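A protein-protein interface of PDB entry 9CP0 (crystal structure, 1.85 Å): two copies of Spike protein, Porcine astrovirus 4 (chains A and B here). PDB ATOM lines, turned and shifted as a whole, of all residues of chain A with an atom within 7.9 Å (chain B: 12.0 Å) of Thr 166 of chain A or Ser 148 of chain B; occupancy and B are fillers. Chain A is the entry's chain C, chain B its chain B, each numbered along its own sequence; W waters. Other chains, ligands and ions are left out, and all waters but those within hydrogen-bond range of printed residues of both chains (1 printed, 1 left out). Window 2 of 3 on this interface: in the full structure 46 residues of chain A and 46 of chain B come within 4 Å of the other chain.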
ATOM      1  N   ALA A  36       9.578  12.777 -21.417  1.00  0.00           N
ATOM      2  CA  ALA A  36       8.881  13.885 -22.048  1.00  0.00           C
ATOM      3  C   ALA A  36       9.903  14.979 -22.312  1.00  0.00           C
ATOM      4  O   ALA A  36      10.675  15.334 -21.415  1.00  0.00           O
ATOM      5  CB  ALA A  36       7.742  14.409 -21.167  1.00  0.00           C
ATOM      6  N   TYR A  52      15.504  19.945 -23.562  1.00  0.00           N
ATOM      7  CA  TYR A  52      14.666  20.630 -22.592  1.00  0.00           C
ATOM      8  C   TYR A  52      14.708  22.142 -22.777  1.00  0.00           C
ATOM      9  O   TYR A  52      14.053  22.865 -22.017  1.00  0.00           O
ATOM     10  CB  TYR A  52      15.081  20.267 -21.158  1.00  0.00           C
ATOM     11  CG  TYR A  52      15.093  18.775 -20.878  1.00  0.00           C
ATOM     12  CD1 TYR A  52      13.910  18.040 -20.888  1.00  0.00           C
ATOM     13  CD2 TYR A  52      16.271  18.110 -20.572  1.00  0.00           C
ATOM     14  CE1 TYR A  52      13.907  16.681 -20.628  1.00  0.00           C
ATOM     15  CE2 TYR A  52      16.280  16.751 -20.301  1.00  0.00           C
ATOM     16  CZ  TYR A  52      15.095  16.046 -20.334  1.00  0.00           C
ATOM     17  OH  TYR A  52      15.099  14.691 -20.076  1.00  0.00           O
ATOM     18  N   ARG A 125       4.958  19.068 -21.186  1.00  0.00           N
ATOM     19  CA  ARG A 125       5.558  18.320 -20.091  1.00  0.00           C
ATOM     20  C   ARG A 125       7.015  18.024 -20.407  1.00  0.00           C
ATOM     21  O   ARG A 125       7.344  17.607 -21.522  1.00  0.00           O
ATOM     22  CB  ARG A 125       4.795  17.012 -19.854  1.00  0.00           C
ATOM     23  CG  ARG A 125       5.362  16.127 -18.737  1.00  0.00           C
ATOM     24  CD  ARG A 125       4.390  15.028 -18.322  1.00  0.00           C
ATOM     25  NE  ARG A 125       4.442  13.882 -19.223  1.00  0.00           N
ATOM     26  CZ  ARG A 125       4.717  12.642 -18.838  1.00  0.00           C
ATOM     27  NH1 ARG A 125       4.956  12.352 -17.572  1.00  0.00           N
ATOM     28  NH2 ARG A 125       4.760  11.674 -19.747  1.00  0.00           N
ATOM     29  N   LEU A 126       7.891  18.265 -19.432  1.00  0.00           N
ATOM     30  CA  LEU A 126       9.272  17.809 -19.485  1.00  0.00           C
ATOM     31  C   LEU A 126       9.515  16.856 -18.327  1.00  0.00           C
ATOM     32  O   LEU A 126       9.087  17.122 -17.199  1.00  0.00           O
ATOM     33  CB  LEU A 126      10.264  18.966 -19.429  1.00  0.00           C
ATOM     34  CG  LEU A 126       9.992  20.168 -20.324  1.00  0.00           C
ATOM     35  CD1 LEU A 126      11.015  21.241 -20.030  1.00  0.00           C
ATOM     36  CD2 LEU A 126      10.076  19.747 -21.780  1.00  0.00           C
ATOM     37  N   ARG A 127      10.173  15.741 -18.619  1.00  0.00           N
ATOM     38  CA  ARG A 127      10.489  14.744 -17.604  1.00  0.00           C
ATOM     39  C   ARG A 127      11.543  13.802 -18.160  1.00  0.00           C
ATOM     40  O   ARG A 127      11.366  13.245 -19.245  1.00  0.00           O
ATOM     41  CB  ARG A 127       9.256  13.951 -17.160  1.00  0.00           C
ATOM     42  CG  ARG A 127       9.615  12.884 -16.106  1.00  0.00           C
ATOM     43  CD  ARG A 127       8.458  12.545 -15.171  1.00  0.00           C
ATOM     44  NE  ARG A 127       8.669  11.307 -14.429  1.00  0.00           N
ATOM     45  CZ  ARG A 127       7.806  10.807 -13.555  1.00  0.00           C
ATOM     46  NH1 ARG A 127       6.651  11.403 -13.309  1.00  0.00           N
ATOM     47  NH2 ARG A 127       8.124   9.700 -12.888  1.00  0.00           N
ATOM     48  N   GLY A 128      12.644  13.641 -17.425  1.00  0.00           N
ATOM     49  CA  GLY A 128      13.687  12.753 -17.873  1.00  0.00           C
ATOM     50  C   GLY A 128      13.374  11.307 -17.553  1.00  0.00           C
ATOM     51  O   GLY A 128      12.475  10.986 -16.776  1.00  0.00           O
ATOM     52  N   HIS A 129      14.136  10.424 -18.191  1.00  0.00           N
ATOM     53  CA  HIS A 129      14.099   9.012 -17.846  1.00  0.00           C
ATOM     54  C   HIS A 129      14.291   8.834 -16.343  1.00  0.00           C
ATOM     55  O   HIS A 129      14.921   9.660 -15.674  1.00  0.00           O
ATOM     56  CB  HIS A 129      15.184   8.259 -18.619  1.00  0.00           C
ATOM     57  CG  HIS A 129      15.045   6.769 -18.557  1.00  0.00           C
ATOM     58  ND1 HIS A 129      15.535   6.023 -17.506  1.00  0.00           N
ATOM     59  CD2 HIS A 129      14.479   5.885 -19.414  1.00  0.00           C
ATOM     60  CE1 HIS A 129      15.270   4.747 -17.715  1.00  0.00           C
ATOM     61  NE2 HIS A 129      14.637   4.635 -18.868  1.00  0.00           N
ATOM     62  N   ASP A 134      19.919  13.206 -17.530  1.00  0.00           N
ATOM     63  CA  ASP A 134      19.836  14.597 -17.954  1.00  0.00           C
ATOM     64  C   ASP A 134      21.015  15.417 -17.464  1.00  0.00           C
ATOM     65  O   ASP A 134      21.292  15.479 -16.259  1.00  0.00           O
ATOM     66  CB  ASP A 134      18.525  15.194 -17.455  1.00  0.00           C
ATOM     67  CG  ASP A 134      17.344  14.390 -17.910  1.00  0.00           C
ATOM     68  OD1 ASP A 134      17.435  13.894 -19.050  1.00  0.00           O
ATOM     69  OD2 ASP A 134      16.379  14.202 -17.134  1.00  0.00           O
ATOM     70  N   PHE A 136      23.103  19.369 -18.430  1.00  0.00           N
ATOM     71  CA  PHE A 136      22.928  20.691 -19.002  1.00  0.00           C
ATOM     72  C   PHE A 136      24.295  21.306 -19.238  1.00  0.00           C
ATOM     73  O   PHE A 136      25.228  21.094 -18.452  1.00  0.00           O
ATOM     74  CB  PHE A 136      22.090  21.576 -18.076  1.00  0.00           C
ATOM     75  CG  PHE A 136      20.704  21.069 -17.878  1.00  0.00           C
ATOM     76  CD1 PHE A 136      20.437  20.108 -16.915  1.00  0.00           C
ATOM     77  CD2 PHE A 136      19.683  21.472 -18.721  1.00  0.00           C
ATOM     78  CE1 PHE A 136      19.165  19.617 -16.749  1.00  0.00           C
ATOM     79  CE2 PHE A 136      18.408  20.983 -18.558  1.00  0.00           C
ATOM     80  CZ  PHE A 136      18.148  20.047 -17.577  1.00  0.00           C
ATOM     81  N   SER A 161      25.837  17.982 -13.160  1.00  0.00           N
ATOM     82  CA  SER A 161      25.899  16.560 -12.851  1.00  0.00           C
ATOM     83  C   SER A 161      24.642  15.859 -13.353  1.00  0.00           C
ATOM     84  O   SER A 161      23.633  16.491 -13.674  1.00  0.00           O
ATOM     85  CB  SER A 161      26.048  16.323 -11.347  1.00  0.00           C
ATOM     86  OG  SER A 161      24.982  16.899 -10.609  1.00  0.00           O
ATOM     87  N   LEU A 162      24.718  14.534 -13.431  1.00  0.00           N
ATOM     88  CA  LEU A 162      23.588  13.756 -13.917  1.00  0.00           C
ATOM     89  C   LEU A 162      22.416  13.868 -12.955  1.00  0.00           C
ATOM     90  O   LEU A 162      22.578  13.726 -11.741  1.00  0.00           O
ATOM     91  CB  LEU A 162      23.975  12.291 -14.094  1.00  0.00           C
ATOM     92  CG  LEU A 162      24.897  11.908 -15.246  1.00  0.00           C
ATOM     93  CD1 LEU A 162      25.645  10.647 -14.876  1.00  0.00           C
ATOM     94  CD2 LEU A 162      24.072  11.666 -16.497  1.00  0.00           C
ATOM     95  N   VAL A 163      21.233  14.141 -13.502  1.00  0.00           N
ATOM     96  CA  VAL A 163      20.001  14.179 -12.729  1.00  0.00           C
ATOM     97  C   VAL A 163      18.910  13.491 -13.531  1.00  0.00           C
ATOM     98  O   VAL A 163      19.045  13.244 -14.731  1.00  0.00           O
ATOM     99  CB  VAL A 163      19.561  15.616 -12.371  1.00  0.00           C
ATOM    100  CG1 VAL A 163      20.634  16.327 -11.559  1.00  0.00           C
ATOM    101  CG2 VAL A 163      19.239  16.394 -13.640  1.00  0.00           C
ATOM    102  N   SER A 164      17.824  13.174 -12.845  1.00  0.00           N
ATOM    103  CA  SER A 164      16.586  12.719 -13.470  1.00  0.00           C
ATOM    104  C   SER A 164      15.582  13.852 -13.351  1.00  0.00           C
ATOM    105  O   SER A 164      14.920  13.995 -12.317  1.00  0.00           O
ATOM    106  CB  SER A 164      16.050  11.456 -12.816  1.00  0.00           C
ATOM    107  OG  SER A 164      14.727  11.237 -13.262  1.00  0.00           O
ATOM    108  N   LEU A 165      15.470  14.640 -14.422  1.00  0.00           N
ATOM    109  CA  LEU A 165      14.653  15.844 -14.426  1.00  0.00           C
ATOM    110  C   LEU A 165      13.255  15.570 -13.897  1.00  0.00           C
ATOM    111  O   LEU A 165      12.508  14.766 -14.464  1.00  0.00           O
ATOM    112  CB  LEU A 165      14.589  16.402 -15.848  1.00  0.00           C
ATOM    113  CG  LEU A 165      14.156  17.860 -15.955  1.00  0.00           C
ATOM    114  CD1 LEU A 165      15.315  18.785 -15.645  1.00  0.00           C
ATOM    115  CD2 LEU A 165      13.615  18.123 -17.350  1.00  0.00           C
ATOM    116  N   THR A 166      12.913  16.239 -12.799  1.00  0.00           N
ATOM    117  CA  THR A 166      11.586  16.129 -12.217  1.00  0.00           C
ATOM    118  C   THR A 166      10.525  16.614 -13.199  1.00  0.00           C
ATOM    119  O   THR A 166      10.737  17.569 -13.958  1.00  0.00           O
ATOM    120  CB  THR A 166      11.503  16.954 -10.935  1.00  0.00           C
ATOM    121  OG1 THR A 166      12.609  16.637 -10.078  1.00  0.00           O
ATOM    122  CG2 THR A 166      10.198  16.687 -10.207  1.00  0.00           C
ATOM    123  N   GLU A 167       9.375  15.945 -13.165  1.00  0.00           N
ATOM    124  CA  GLU A 167       8.254  16.315 -14.015  1.00  0.00           C
ATOM    125  C   GLU A 167       7.889  17.786 -13.826  1.00  0.00           C
ATOM    126  O   GLU A 167       7.916  18.313 -12.709  1.00  0.00           O
ATOM    127  CB  GLU A 167       7.051  15.430 -13.692  1.00  0.00           C
ATOM    128  CG  GLU A 167       5.908  15.500 -14.700  1.00  0.00           C
ATOM    129  CD  GLU A 167       5.035  14.266 -14.653  1.00  0.00           C
ATOM    130  OE1 GLU A 167       5.360  13.273 -15.333  1.00  0.00           O
ATOM    131  OE2 GLU A 167       4.030  14.277 -13.914  1.00  0.00           O
ATOM    132  N   ARG A 168       7.550  18.449 -14.930  1.00  0.00           N
ATOM    133  CA  ARG A 168       7.205  19.862 -14.880  1.00  0.00           C
ATOM    134  C   ARG A 168       6.424  20.229 -16.129  1.00  0.00           C
ATOM    135  O   ARG A 168       6.467  19.529 -17.145  1.00  0.00           O
ATOM    136  CB  ARG A 168       8.452  20.742 -14.754  1.00  0.00           C
ATOM    137  CG  ARG A 168       9.454  20.568 -15.877  1.00  0.00           C
ATOM    138  CD  ARG A 168      10.758  21.286 -15.547  1.00  0.00           C
ATOM    139  NE  ARG A 168      10.607  22.735 -15.564  1.00  0.00           N
ATOM    140  CZ  ARG A 168      11.156  23.555 -14.679  1.00  0.00           C
ATOM    141  NH1 ARG A 168      11.879  23.099 -13.671  1.00  0.00           N
ATOM    142  NH2 ARG A 168      10.971  24.867 -14.808  1.00  0.00           N
ATOM    143  N   GLN A 169       5.712  21.347 -16.037  1.00  0.00           N
ATOM    144  CA  GLN A 169       4.902  21.872 -17.123  1.00  0.00           C
ATOM    145  C   GLN A 169       5.500  23.193 -17.589  1.00  0.00           C
ATOM    146  O   GLN A 169       5.812  24.060 -16.765  1.00  0.00           O
ATOM    147  CB  GLN A 169       3.451  22.071 -16.667  1.00  0.00           C
ATOM    148  CG  GLN A 169       2.539  20.823 -16.553  1.00  0.00           C
ATOM    149  CD  GLN A 169       2.806  19.722 -17.577  1.00  0.00           C
ATOM    150  OE1 GLN A 169       3.853  19.081 -17.572  1.00  0.00           O
ATOM    151  NE2 GLN A 169       1.846  19.510 -18.472  1.00  0.00           N
ATOM    152  N   LEU B 143      25.301  29.345 -14.832  1.00  0.00           N
ATOM    153  CA  LEU B 143      24.261  28.325 -14.853  1.00  0.00           C
ATOM    154  C   LEU B 143      24.045  27.840 -13.430  1.00  0.00           C
ATOM    155  O   LEU B 143      24.948  27.259 -12.826  1.00  0.00           O
ATOM    156  CB  LEU B 143      24.655  27.178 -15.779  1.00  0.00           C
ATOM    157  CG  LEU B 143      23.532  26.208 -16.169  1.00  0.00           C
ATOM    158  CD1 LEU B 143      22.702  26.764 -17.311  1.00  0.00           C
ATOM    159  CD2 LEU B 143      24.100  24.848 -16.552  1.00  0.00           C
ATOM    160  N   SER B 144      22.871  28.111 -12.877  1.00  0.00           N
ATOM    161  CA  SER B 144      22.526  27.658 -11.540  1.00  0.00           C
ATOM    162  C   SER B 144      21.464  26.576 -11.631  1.00  0.00           C
ATOM    163  O   SER B 144      20.551  26.648 -12.462  1.00  0.00           O
ATOM    164  CB  SER B 144      22.020  28.800 -10.653  1.00  0.00           C
ATOM    165  OG  SER B 144      20.825  29.363 -11.156  1.00  0.00           O
ATOM    166  N   MET B 145      21.588  25.580 -10.767  1.00  0.00           N
ATOM    167  CA  MET B 145      20.674  24.452 -10.734  1.00  0.00           C
ATOM    168  C   MET B 145      20.253  24.192  -9.299  1.00  0.00           C
ATOM    169  O   MET B 145      21.102  24.055  -8.411  1.00  0.00           O
ATOM    170  CB  MET B 145      21.325  23.211 -11.319  1.00  0.00           C
ATOM    171  CG  MET B 145      20.354  22.246 -11.939  1.00  0.00           C
ATOM    172  SD  MET B 145      21.187  21.428 -13.291  1.00  0.00           S
ATOM    173  CE  MET B 145      20.187  19.948 -13.410  1.00  0.00           C
ATOM    174  N   SER B 146      18.949  24.139  -9.073  1.00  0.00           N
ATOM    175  CA  SER B 146      18.377  23.813  -7.774  1.00  0.00           C
ATOM    176  C   SER B 146      17.794  22.406  -7.887  1.00  0.00           C
ATOM    177  O   SER B 146      16.663  22.219  -8.341  1.00  0.00           O
ATOM    178  CB  SER B 146      17.329  24.843  -7.370  1.00  0.00           C
ATOM    179  OG  SER B 146      16.558  24.396  -6.269  1.00  0.00           O
ATOM    180  N   GLY B 147      18.591  21.411  -7.495  1.00  0.00           N
ATOM    181  CA  GLY B 147      18.144  20.033  -7.499  1.00  0.00           C
ATOM    182  C   GLY B 147      18.105  19.400  -8.875  1.00  0.00           C
ATOM    183  O   GLY B 147      19.029  19.576  -9.677  1.00  0.00           O
ATOM    184  N   SER B 148      17.045  18.650  -9.152  1.00  0.00           N
ATOM    185  CA  SER B 148      16.859  17.995 -10.449  1.00  0.00           C
ATOM    186  C   SER B 148      15.867  18.755 -11.318  1.00  0.00           C
ATOM    187  O   SER B 148      14.934  18.170 -11.865  1.00  0.00           O
ATOM    188  CB  SER B 148      16.404  16.553 -10.249  1.00  0.00           C
ATOM    189  OG  SER B 148      15.229  16.507  -9.455  1.00  0.00           O
ATOM    190  N   ASN B 149      16.045  20.064 -11.470  1.00  0.00           N
ATOM    191  CA  ASN B 149      15.119  20.863 -12.262  1.00  0.00           C
ATOM    192  C   ASN B 149      15.875  21.646 -13.323  1.00  0.00           C
ATOM    193  O   ASN B 149      17.109  21.642 -13.374  1.00  0.00           O
ATOM    194  CB  ASN B 149      14.286  21.802 -11.380  1.00  0.00           C
ATOM    195  CG  ASN B 149      13.514  21.060 -10.309  1.00  0.00           C
ATOM    196  OD1 ASN B 149      12.286  20.928 -10.392  1.00  0.00           O
ATOM    197  ND2 ASN B 149      14.223  20.558  -9.307  1.00  0.00           N
ATOM    198  N   LEU B 150      15.108  22.323 -14.177  1.00  0.00           N
ATOM    199  CA  LEU B 150      15.691  23.115 -15.244  1.00  0.00           C
ATOM    200  C   LEU B 150      16.554  24.229 -14.663  1.00  0.00           C
ATOM    201  O   LEU B 150      16.149  24.893 -13.705  1.00  0.00           O
ATOM    202  CB  LEU B 150      14.608  23.725 -16.123  1.00  0.00           C
ATOM    203  CG  LEU B 150      13.957  22.791 -17.135  1.00  0.00           C
ATOM    204  CD1 LEU B 150      12.834  23.538 -17.835  1.00  0.00           C
ATOM    205  CD2 LEU B 150      14.993  22.297 -18.126  1.00  0.00           C
ATOM    206  N   PRO B 151      17.730  24.469 -15.232  1.00  0.00           N
ATOM    207  CA  PRO B 151      18.621  25.494 -14.691  1.00  0.00           C
ATOM    208  C   PRO B 151      18.164  26.891 -15.077  1.00  0.00           C
ATOM    209  O   PRO B 151      17.401  27.093 -16.023  1.00  0.00           O
ATOM    210  CB  PRO B 151      19.970  25.162 -15.336  1.00  0.00           C
ATOM    211  CG  PRO B 151      19.602  24.467 -16.612  1.00  0.00           C
ATOM    212  CD  PRO B 151      18.354  23.714 -16.331  1.00  0.00           C
ATOM    213  N   THR B 152      18.646  27.860 -14.309  1.00  0.00           N
ATOM    214  CA  THR B 152      18.438  29.272 -14.591  1.00  0.00           C
ATOM    215  C   THR B 152      19.792  29.962 -14.704  1.00  0.00           C
ATOM    216  O   THR B 152      20.840  29.369 -14.431  1.00  0.00           O
ATOM    217  CB  THR B 152      17.608  29.953 -13.495  1.00  0.00           C
ATOM    218  OG1 THR B 152      18.280  29.815 -12.237  1.00  0.00           O
ATOM    219  CG2 THR B 152      16.235  29.318 -13.390  1.00  0.00           C
HETATM  220  O   HOH W   1      11.850  19.789 -12.701  1.00  0.00           O
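The side-chain hydroxyl (OG1) of Thr 166 of chain A sits at hydrogen-bond distance from the side-chain hydroxyl (OG) of Ser 148 of chain B (2.7 Å).
NH1 of Arg 168 of chain A lies close to N of Leu 150 of chain B (3.4 Å).
The side-chain hydroxyl of Ser 164 of chain A lies within hydrogen-bond range of the backbone carbonyl oxygen of His 129 of chain A.
O of Arg 168 of chain A lies within hydrogen-bond range of N of Leu 126 of chain A (3.0 Å).
N of Asp 134 of chain A is in hydrogen-bond range of O of Val 163 of chain A (2.9 Å).
The backbone NH (N) of Leu 165 of chain A sits at hydrogen-bond distance from the side-chain carboxylate (OD2) of Asp 134 of chain A, at 2.9 Å.
The backbone NH of Gly 128 of chain A lies within hydrogen-bond range of the backbone carbonyl oxygen of Leu 165 of chain A (3.2 Å).
O of Ser 146 of chain B lies within hydrogen-bond range of ND2 of Asn 149 of chain B, 3.1 Å away.
Among the printed residues, pairs that only touch across the chains: Tyr 52 of chain A with Leu 150 of chain B, Leu 126 of chain A with Leu 150 of chain B, Phe 136 of chain A with Met 145 of chain B, Phe 136 of chain A with Leu 150 of chain B, Phe 136 of chain A with Pro 151 of chain B, Val 163 of chain A with Met 145 of chain B, Val 163 of chain A with Ser 148 of chain B, Ser 164 of chain A with Ser 148 of chain B, Leu 165 of chain A with Ser 148 of chain B, Leu 165 of chain A with Asn 149 of chain B, Leu 165 of chain A with Leu 150 of chain B and Arg 168 of chain A with Asn 149 of chain B.
Printed residues of chain B within 4 Å of Tyr 52 of chain A: Leu 150.
Of the printed residues of chain B, Leu 126 of chain A touches Leu 150.
No residue of chain B comes within 4 Å of Arg 127 of chain A.
No residue of chain B comes within 4 Å of Gly 128 of chain A.
Ser 161 of chain A touches none of the printed residues of chain B.
Of chain B, only Met 145 and Ser 148 come within 4 Å of Val 163 of chain A.
Ser 164 of chain A touches just one residue of chain B: Ser 148.
Printed residues of chain B within 4 Å of Leu 165 of chain A: Ser 148 (3.5 Å), Asn 149 (3.7 Å) and Leu 150 (3.8 Å).
Printed residues of chain B within 4 Å of Thr 166 of chain A: Ser 148 (2.7 Å).
Printed residues of chain A within 4 Å of Met 145 of chain B: Phe 136 and Val 163.
No residue of chain A comes within 4 Å of Gly 147 of chain B.
Of the printed residues of chain A, Ser 148 of chain B touches Val 163 (3.9 Å), Ser 164 (3.6 Å), Leu 165 (3.5 Å) and Thr 166 (2.7 Å).
Of the printed residues of chain A, Asn 149 of chain B touches Leu 165 (3.7 Å) and Arg 168 (3.6 Å).
Of the printed residues of chain A, Pro 151 of chain B touches Phe 136.
The nearest residue of chain B that does not touch Thr 166 of chain A is Asn 149 of chain B (4.1 Å).
The nearest residue of chain A that does not touch Ser 148 of chain B is Arg 168 of chain A (6.1 Å).
Printed residues of chain A that touch a printed residue of chain B: Tyr 52, Leu 126, Phe 136, Val 163, Ser 164, Leu 165, Thr 166 and Arg 168.
Hydrophobic or aromatic side chains of chain A within 4 Å of the printed part of chain B: Tyr 52, Leu 126, Phe 136, Val 163 and Leu 165.
Printed residues of chain B that touch a printed residue of chain A: Met 145, Ser 148, Asn 149, Leu 150 and Pro 151.
Hydrophobic or aromatic side chains of chain B that line the printed part of chain A: Met 145, Leu 150 and Pro 151.
Among the printed residues, no Asp or Glu carboxylate lies within 4 Å of a Lys or Arg side-chain nitrogen of the other chain.
No position is printed for both chains.
Of the 14 pairs that touch across the chains among the printed residues, none has its exchanged pair printed and touching as well.
Water W1 lies within hydrogen-bond range of the side-chain amide oxygen (OD1) of Asn 149 of chain B (2.6 Å), the backbone carbonyl oxygen (O) of Thr 166 of chain A (2.8 Å) and the guanidinium group (NH1) of Arg 168 of chain A (3.4 Å).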
